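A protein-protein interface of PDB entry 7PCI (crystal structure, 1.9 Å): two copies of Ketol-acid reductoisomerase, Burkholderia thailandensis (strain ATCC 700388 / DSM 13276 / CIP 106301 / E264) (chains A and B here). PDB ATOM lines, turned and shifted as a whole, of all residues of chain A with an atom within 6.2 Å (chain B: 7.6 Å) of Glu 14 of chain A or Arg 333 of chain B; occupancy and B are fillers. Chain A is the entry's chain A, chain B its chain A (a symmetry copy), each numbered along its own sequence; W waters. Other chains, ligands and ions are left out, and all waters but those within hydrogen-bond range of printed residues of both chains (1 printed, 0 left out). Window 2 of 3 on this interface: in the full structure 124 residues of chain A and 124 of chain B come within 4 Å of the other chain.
The backbone carbonyl oxygen (O) of Ala 182 of chain A is in hydrogen-bond range of the backbone NH (N) of Arg 333 of chain B (2.8 Å). The guanidinium group of Arg 333 of chain B is in hydrogen-bond range of the side-chain amide oxygen of Gln 12 of chain A (2.7 Å). The backbone carbonyl oxygen (O) of Ala 331 of chain B is in hydrogen-bond range of the side-chain amide nitrogen (NE2) of Gln 12 of chain A (2.8 Å). The guanidinium group (NH1) of Arg 333 of chain B is in salt-bridge range of the side-chain carboxylate (OE1) of Glu 14 of chain A, 2.9 Å away.
NE2 of Gln 12 of chain A is in hydrogen-bond range of O of Ala 182 of chain A (3.3 Å). A ring nitrogen (ND1) of His 15 of chain A is in hydrogen-bond range of the backbone NH of Gln 12 of chain A, at 3.0 Å. The backbone carbonyl oxygen of Phe 332 of chain B lies within hydrogen-bond range of the guanidinium group of Arg 329 of chain B, at 2.8 Å.
Among the printed residues, merely in contact across the chains: Ala 182 of chain A with Phe 332 of chain B, Arg 181 of chain A with Arg 333 of chain B, Gly 183 of chain A with Phe 332 of chain B, Pro 153 of chain A with Phe 332 of chain B and Pro 153 of chain A with Ser 235 of chain B.
Of the printed residues of chain B, Gln 12 of chain A touches Ala 331 (2.8 Å) and Arg 333 (2.7 Å). Glu 14 of chain A touches just one residue of chain B: Arg 333 (2.9 Å). Thr 180 of chain A touches none of the printed residues of chain B. Of the printed residues of chain B, Arg 181 of chain A touches Arg 333 (3.4 Å). Printed residues of chain A within 4 Å of Ala 331 of chain B: Gln 12. Of the printed residues of chain A, Phe 332 of chain B touches Pro 153 (3.997 Å), Ala 182 (3.4 Å) and Gly 183 (3.6 Å). The nearest printed residue of chain B that does not touch Glu 14 of chain A is Ala 331 of chain B (8.6 Å).
Hydrophobic or aromatic side chains of chain B within 4 Å of the printed part of chain A: Phe 332. Along chain B the printed residues that touch a printed residue of chain A span positions 235 to 333. Printed residues of chain A that touch a printed residue of chain B: Gln 12, Glu 14, Pro 153, Arg 181, Ala 182 and Gly 183. Hydrophobic or aromatic side chains of chain A that line the printed part of chain B: Pro 153 and Ala 182. Among the printed residues, 9 pairs touch across the chains.
No position is printed for both chains.
Water W1 lies within hydrogen-bond range of the backbone carbonyl oxygen of Thr 180 of chain A, the backbone NH of Asp 13 of chain A and the guanidinium group of Arg 333 of chain B.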
ATOM      1  N   GLN A  12     -12.798  20.148  18.575  1.00  0.00           N
ATOM      2  CA  GLN A  12     -11.728  20.349  17.566  1.00  0.00           C
ATOM      3  C   GLN A  12     -12.370  21.056  16.367  1.00  0.00           C
ATOM      4  O   GLN A  12     -13.563  21.395  16.474  1.00  0.00           O
ATOM      5  CB  GLN A  12     -11.048  19.009  17.281  1.00  0.00           C
ATOM      6  CG  GLN A  12     -10.479  18.377  18.548  1.00  0.00           C
ATOM      7  CD  GLN A  12      -9.727  17.087  18.327  1.00  0.00           C
ATOM      8  OE1 GLN A  12      -9.750  16.502  17.249  1.00  0.00           O
ATOM      9  NE2 GLN A  12      -9.053  16.627  19.370  1.00  0.00           N
ATOM     10  N   ASP A  13     -11.603  21.312  15.301  1.00  0.00           N
ATOM     11  CA  ASP A  13     -12.002  22.197  14.172  1.00  0.00           C
ATOM     12  C   ASP A  13     -13.386  21.793  13.645  1.00  0.00           C
ATOM     13  O   ASP A  13     -14.196  22.700  13.387  1.00  0.00           O
ATOM     14  CB  ASP A  13     -10.960  22.192  13.047  1.00  0.00           C
ATOM     15  CG  ASP A  13      -9.791  23.141  13.258  1.00  0.00           C
ATOM     16  OD1 ASP A  13      -9.847  23.961  14.196  1.00  0.00           O
ATOM     17  OD2 ASP A  13      -8.831  23.052  12.476  1.00  0.00           O
ATOM     18  N   GLU A  14     -13.650  20.490  13.506  1.00  0.00           N
ATOM     19  CA  GLU A  14     -14.883  19.965  12.854  1.00  0.00           C
ATOM     20  C   GLU A  14     -16.107  20.157  13.765  1.00  0.00           C
ATOM     21  O   GLU A  14     -17.228  19.946  13.273  1.00  0.00           O
ATOM     22  CB  GLU A  14     -14.715  18.498  12.447  1.00  0.00           C
ATOM     23  CG  GLU A  14     -14.656  17.520  13.609  1.00  0.00           C
ATOM     24  CD  GLU A  14     -13.258  17.174  14.087  1.00  0.00           C
ATOM     25  OE1 GLU A  14     -12.390  18.068  14.071  1.00  0.00           O
ATOM     26  OE2 GLU A  14     -13.043  16.011  14.466  1.00  0.00           O
ATOM     27  N   HIS A  15     -15.909  20.531  15.035  1.00  0.00           N
ATOM     28  CA  HIS A  15     -16.996  20.712  16.037  1.00  0.00           C
ATOM     29  C   HIS A  15     -17.336  22.196  16.237  1.00  0.00           C
ATOM     30  O   HIS A  15     -18.230  22.480  17.058  1.00  0.00           O
ATOM     31  CB  HIS A  15     -16.611  20.064  17.374  1.00  0.00           C
ATOM     32  CG  HIS A  15     -16.152  18.652  17.254  1.00  0.00           C
ATOM     33  ND1 HIS A  15     -14.911  18.243  17.695  1.00  0.00           N
ATOM     34  CD2 HIS A  15     -16.752  17.557  16.741  1.00  0.00           C
ATOM     35  CE1 HIS A  15     -14.766  16.955  17.467  1.00  0.00           C
ATOM     36  NE2 HIS A  15     -15.880  16.512  16.880  1.00  0.00           N
ATOM     37  N   ALA A  16     -16.664  23.110  15.531  1.00  0.00           N
ATOM     38  CA  ALA A  16     -16.810  24.571  15.723  1.00  0.00           C
ATOM     39  C   ALA A  16     -16.826  25.283  14.367  1.00  0.00           C
ATOM     40  O   ALA A  16     -15.930  25.021  13.550  1.00  0.00           O
ATOM     41  CB  ALA A  16     -15.702  25.088  16.607  1.00  0.00           C
ATOM     42  N   GLY A 151      -2.102  24.640  16.725  1.00  0.00           N
ATOM     43  CA  GLY A 151      -2.599  25.416  17.871  1.00  0.00           C
ATOM     44  C   GLY A 151      -2.318  24.695  19.168  1.00  0.00           C
ATOM     45  O   GLY A 151      -1.884  23.529  19.111  1.00  0.00           O
ATOM     46  N   PRO A 153      -3.974  23.754  23.254  1.00  0.00           N
ATOM     47  CA  PRO A 153      -5.291  23.519  23.837  1.00  0.00           C
ATOM     48  C   PRO A 153      -5.812  24.773  24.551  1.00  0.00           C
ATOM     49  O   PRO A 153      -5.044  25.685  24.782  1.00  0.00           O
ATOM     50  CB  PRO A 153      -5.079  22.368  24.835  1.00  0.00           C
ATOM     51  CG  PRO A 153      -3.704  21.810  24.508  1.00  0.00           C
ATOM     52  CD  PRO A 153      -2.924  22.958  23.904  1.00  0.00           C
ATOM     53  N   ARG A 175     -11.690  28.634  17.406  1.00  0.00           N
ATOM     54  CA  ARG A 175     -11.270  28.061  16.101  1.00  0.00           C
ATOM     55  C   ARG A 175     -10.466  29.105  15.319  1.00  0.00           C
ATOM     56  O   ARG A 175      -9.431  28.727  14.742  1.00  0.00           O
ATOM     57  CB  ARG A 175     -12.453  27.576  15.259  1.00  0.00           C
ATOM     58  CG  ARG A 175     -11.998  26.927  13.961  1.00  0.00           C
ATOM     59  CD  ARG A 175     -13.099  26.363  13.097  1.00  0.00           C
ATOM     60  NE  ARG A 175     -12.561  26.050  11.780  1.00  0.00           N
ATOM     61  CZ  ARG A 175     -13.244  25.488  10.789  1.00  0.00           C
ATOM     62  NH1 ARG A 175     -14.516  25.165  10.949  1.00  0.00           N
ATOM     63  NH2 ARG A 175     -12.645  25.252   9.636  1.00  0.00           N
ATOM     64  N   THR A 180      -8.822  25.023  18.641  1.00  0.00           N
ATOM     65  CA  THR A 180      -9.589  23.807  18.255  1.00  0.00           C
ATOM     66  C   THR A 180      -8.733  22.878  17.383  1.00  0.00           C
ATOM     67  O   THR A 180      -9.149  21.729  17.189  1.00  0.00           O
ATOM     68  CB  THR A 180     -10.907  24.166  17.560  1.00  0.00           C
ATOM     69  OG1 THR A 180     -10.620  25.040  16.468  1.00  0.00           O
ATOM     70  CG2 THR A 180     -11.902  24.803  18.504  1.00  0.00           C
ATOM     71  N   ARG A 181      -7.584  23.341  16.881  1.00  0.00           N
ATOM     72  CA  ARG A 181      -6.626  22.493  16.118  1.00  0.00           C
ATOM     73  C   ARG A 181      -6.018  21.433  17.043  1.00  0.00           C
ATOM     74  O   ARG A 181      -5.652  20.356  16.531  1.00  0.00           O
ATOM     75  CB  ARG A 181      -5.533  23.349  15.475  1.00  0.00           C
ATOM     76  CG  ARG A 181      -6.053  24.255  14.371  1.00  0.00           C
ATOM     77  CD  ARG A 181      -5.085  25.370  14.057  1.00  0.00           C
ATOM     78  NE  ARG A 181      -5.628  26.298  13.079  1.00  0.00           N
ATOM     79  CZ  ARG A 181      -4.923  27.226  12.438  1.00  0.00           C
ATOM     80  NH1 ARG A 181      -3.627  27.361  12.668  1.00  0.00           N
ATOM     81  NH2 ARG A 181      -5.522  28.021  11.568  1.00  0.00           N
ATOM     82  N   ALA A 182      -5.910  21.735  18.341  1.00  0.00           N
ATOM     83  CA  ALA A 182      -5.477  20.800  19.406  1.00  0.00           C
ATOM     84  C   ALA A 182      -6.711  20.240  20.123  1.00  0.00           C
ATOM     85  O   ALA A 182      -6.900  19.009  20.119  1.00  0.00           O
ATOM     86  CB  ALA A 182      -4.554  21.502  20.373  1.00  0.00           C
ATOM     87  N   GLY A 183      -7.519  21.124  20.712  1.00  0.00           N
ATOM     88  CA  GLY A 183      -8.761  20.768  21.420  1.00  0.00           C
ATOM     89  C   GLY A 183      -9.134  21.823  22.444  1.00  0.00           C
ATOM     90  O   GLY A 183      -8.224  22.342  23.113  1.00  0.00           O
ATOM     91  N   GLY B 234       1.643  18.247  29.317  1.00  0.00           N
ATOM     92  CA  GLY B 234       0.878  17.707  28.174  1.00  0.00           C
ATOM     93  C   GLY B 234       0.506  18.759  27.137  1.00  0.00           C
ATOM     94  O   GLY B 234       0.379  18.395  25.944  1.00  0.00           O
ATOM     95  N   SER B 235       0.320  20.012  27.562  1.00  0.00           N
ATOM     96  CA  SER B 235      -0.047  21.155  26.684  1.00  0.00           C
ATOM     97  C   SER B 235       1.141  21.547  25.799  1.00  0.00           C
ATOM     98  O   SER B 235       0.903  22.170  24.749  1.00  0.00           O
ATOM     99  CB  SER B 235      -0.518  22.328  27.497  1.00  0.00           C
ATOM    100  OG  SER B 235       0.527  22.810  28.328  1.00  0.00           O
ATOM    101  N   VAL B 328      -5.071  11.666  27.241  1.00  0.00           N
ATOM    102  CA  VAL B 328      -4.969  13.085  26.783  1.00  0.00           C
ATOM    103  C   VAL B 328      -4.644  13.100  25.284  1.00  0.00           C
ATOM    104  O   VAL B 328      -5.322  13.837  24.549  1.00  0.00           O
ATOM    105  CB  VAL B 328      -3.930  13.895  27.584  1.00  0.00           C
ATOM    106  CG1 VAL B 328      -3.570  15.202  26.887  1.00  0.00           C
ATOM    107  CG2 VAL B 328      -4.406  14.171  29.002  1.00  0.00           C
ATOM    108  N   ARG B 329      -3.643  12.324  24.856  1.00  0.00           N
ATOM    109  CA  ARG B 329      -3.104  12.388  23.471  1.00  0.00           C
ATOM    110  C   ARG B 329      -4.134  11.826  22.483  1.00  0.00           C
ATOM    111  O   ARG B 329      -4.093  12.230  21.309  1.00  0.00           O
ATOM    112  CB  ARG B 329      -1.757  11.667  23.362  1.00  0.00           C
ATOM    113  CG  ARG B 329      -1.021  11.928  22.052  1.00  0.00           C
ATOM    114  CD  ARG B 329      -0.866  13.403  21.715  1.00  0.00           C
ATOM    115  NE  ARG B 329      -0.309  14.187  22.819  1.00  0.00           N
ATOM    116  CZ  ARG B 329      -0.846  15.285  23.358  1.00  0.00           C
ATOM    117  NH1 ARG B 329      -1.987  15.786  22.910  1.00  0.00           N
ATOM    118  NH2 ARG B 329      -0.226  15.889  24.360  1.00  0.00           N
ATOM    119  N   ALA B 330      -5.022  10.940  22.944  1.00  0.00           N
ATOM    120  CA  ALA B 330      -6.163  10.400  22.167  1.00  0.00           C
ATOM    121  C   ALA B 330      -7.203  11.503  21.934  1.00  0.00           C
ATOM    122  O   ALA B 330      -7.801  11.525  20.840  1.00  0.00           O
ATOM    123  CB  ALA B 330      -6.774   9.225  22.890  1.00  0.00           C
ATOM    124  N   ALA B 331      -7.395  12.384  22.923  1.00  0.00           N
ATOM    125  CA  ALA B 331      -8.487  13.386  22.978  1.00  0.00           C
ATOM    126  C   ALA B 331      -8.023  14.749  22.446  1.00  0.00           C
ATOM    127  O   ALA B 331      -8.881  15.501  21.941  1.00  0.00           O
ATOM    128  CB  ALA B 331      -9.000  13.493  24.392  1.00  0.00           C
ATOM    129  N   PHE B 332      -6.731  15.071  22.570  1.00  0.00           N
ATOM    130  CA  PHE B 332      -6.132  16.346  22.092  1.00  0.00           C
ATOM    131  C   PHE B 332      -5.107  16.051  20.994  1.00  0.00           C
ATOM    132  O   PHE B 332      -4.201  15.230  21.231  1.00  0.00           O
ATOM    133  CB  PHE B 332      -5.474  17.109  23.243  1.00  0.00           C
ATOM    134  CG  PHE B 332      -6.430  17.617  24.293  1.00  0.00           C
ATOM    135  CD1 PHE B 332      -6.791  16.818  25.366  1.00  0.00           C
ATOM    136  CD2 PHE B 332      -6.958  18.896  24.213  1.00  0.00           C
ATOM    137  CE1 PHE B 332      -7.663  17.287  26.334  1.00  0.00           C
ATOM    138  CE2 PHE B 332      -7.828  19.366  25.185  1.00  0.00           C
ATOM    139  CZ  PHE B 332      -8.182  18.558  26.241  1.00  0.00           C
ATOM    140  N   ARG B 333      -5.246  16.708  19.837  1.00  0.00           N
ATOM    141  CA  ARG B 333      -4.244  16.661  18.739  1.00  0.00           C
ATOM    142  C   ARG B 333      -3.042  17.517  19.145  1.00  0.00           C
ATOM    143  O   ARG B 333      -3.257  18.617  19.689  1.00  0.00           O
ATOM    144  CB  ARG B 333      -4.832  17.166  17.418  1.00  0.00           C
ATOM    145  CG  ARG B 333      -6.035  16.375  16.933  1.00  0.00           C
ATOM    146  CD  ARG B 333      -6.400  16.714  15.500  1.00  0.00           C
ATOM    147  NE  ARG B 333      -7.841  16.664  15.292  1.00  0.00           N
ATOM    148  CZ  ARG B 333      -8.463  16.992  14.165  1.00  0.00           C
ATOM    149  NH1 ARG B 333      -9.783  16.912  14.102  1.00  0.00           N
ATOM    150  NH2 ARG B 333      -7.775  17.401  13.112  1.00  0.00           N
ATOM    151  N   PHE B 334      -1.828  17.024  18.892  1.00  0.00           N
ATOM    152  CA  PHE B 334      -0.557  17.719  19.218  1.00  0.00           C
ATOM    153  C   PHE B 334       0.105  18.204  17.928  1.00  0.00           C
ATOM    154  O   PHE B 334       0.062  17.514  16.913  1.00  0.00           O
ATOM    155  CB  PHE B 334       0.355  16.800  20.032  1.00  0.00           C
ATOM    156  CG  PHE B 334       1.514  17.518  20.670  1.00  0.00           C
ATOM    157  CD1 PHE B 334       1.360  18.171  21.884  1.00  0.00           C
ATOM    158  CD2 PHE B 334       2.743  17.582  20.034  1.00  0.00           C
ATOM    159  CE1 PHE B 334       2.421  18.853  22.459  1.00  0.00           C
ATOM    160  CE2 PHE B 334       3.803  18.263  20.610  1.00  0.00           C
ATOM    161  CZ  PHE B 334       3.641  18.897  21.821  1.00  0.00           C
ATOM    162  N   PRO B 335       0.720  19.413  17.927  1.00  0.00           N
ATOM    163  CA  PRO B 335       1.418  19.926  16.745  1.00  0.00           C
ATOM    164  C   PRO B 335       2.736  19.186  16.467  1.00  0.00           C
ATOM    165  O   PRO B 335       3.781  19.674  16.849  1.00  0.00           O
ATOM    166  CB  PRO B 335       1.660  21.403  17.096  1.00  0.00           C
ATOM    167  CG  PRO B 335       1.733  21.425  18.606  1.00  0.00           C
ATOM    168  CD  PRO B 335       0.750  20.364  19.051  1.00  0.00           C
ATOM    169  N   THR B 336       2.648  18.034  15.799  1.00  0.00           N
ATOM    170  CA  THR B 336       3.795  17.153  15.450  1.00  0.00           C
ATOM    171  C   THR B 336       4.393  17.577  14.104  1.00  0.00           C
ATOM    172  O   THR B 336       3.617  17.982  13.219  1.00  0.00           O
ATOM    173  CB  THR B 336       3.364  15.682  15.389  1.00  0.00           C
ATOM    174  OG1 THR B 336       2.424  15.533  14.325  1.00  0.00           O
ATOM    175  CG2 THR B 336       2.752  15.197  16.684  1.00  0.00           C
HETATM  176  O   HOH W   1      -8.825  20.079  14.801  1.00  0.00           O
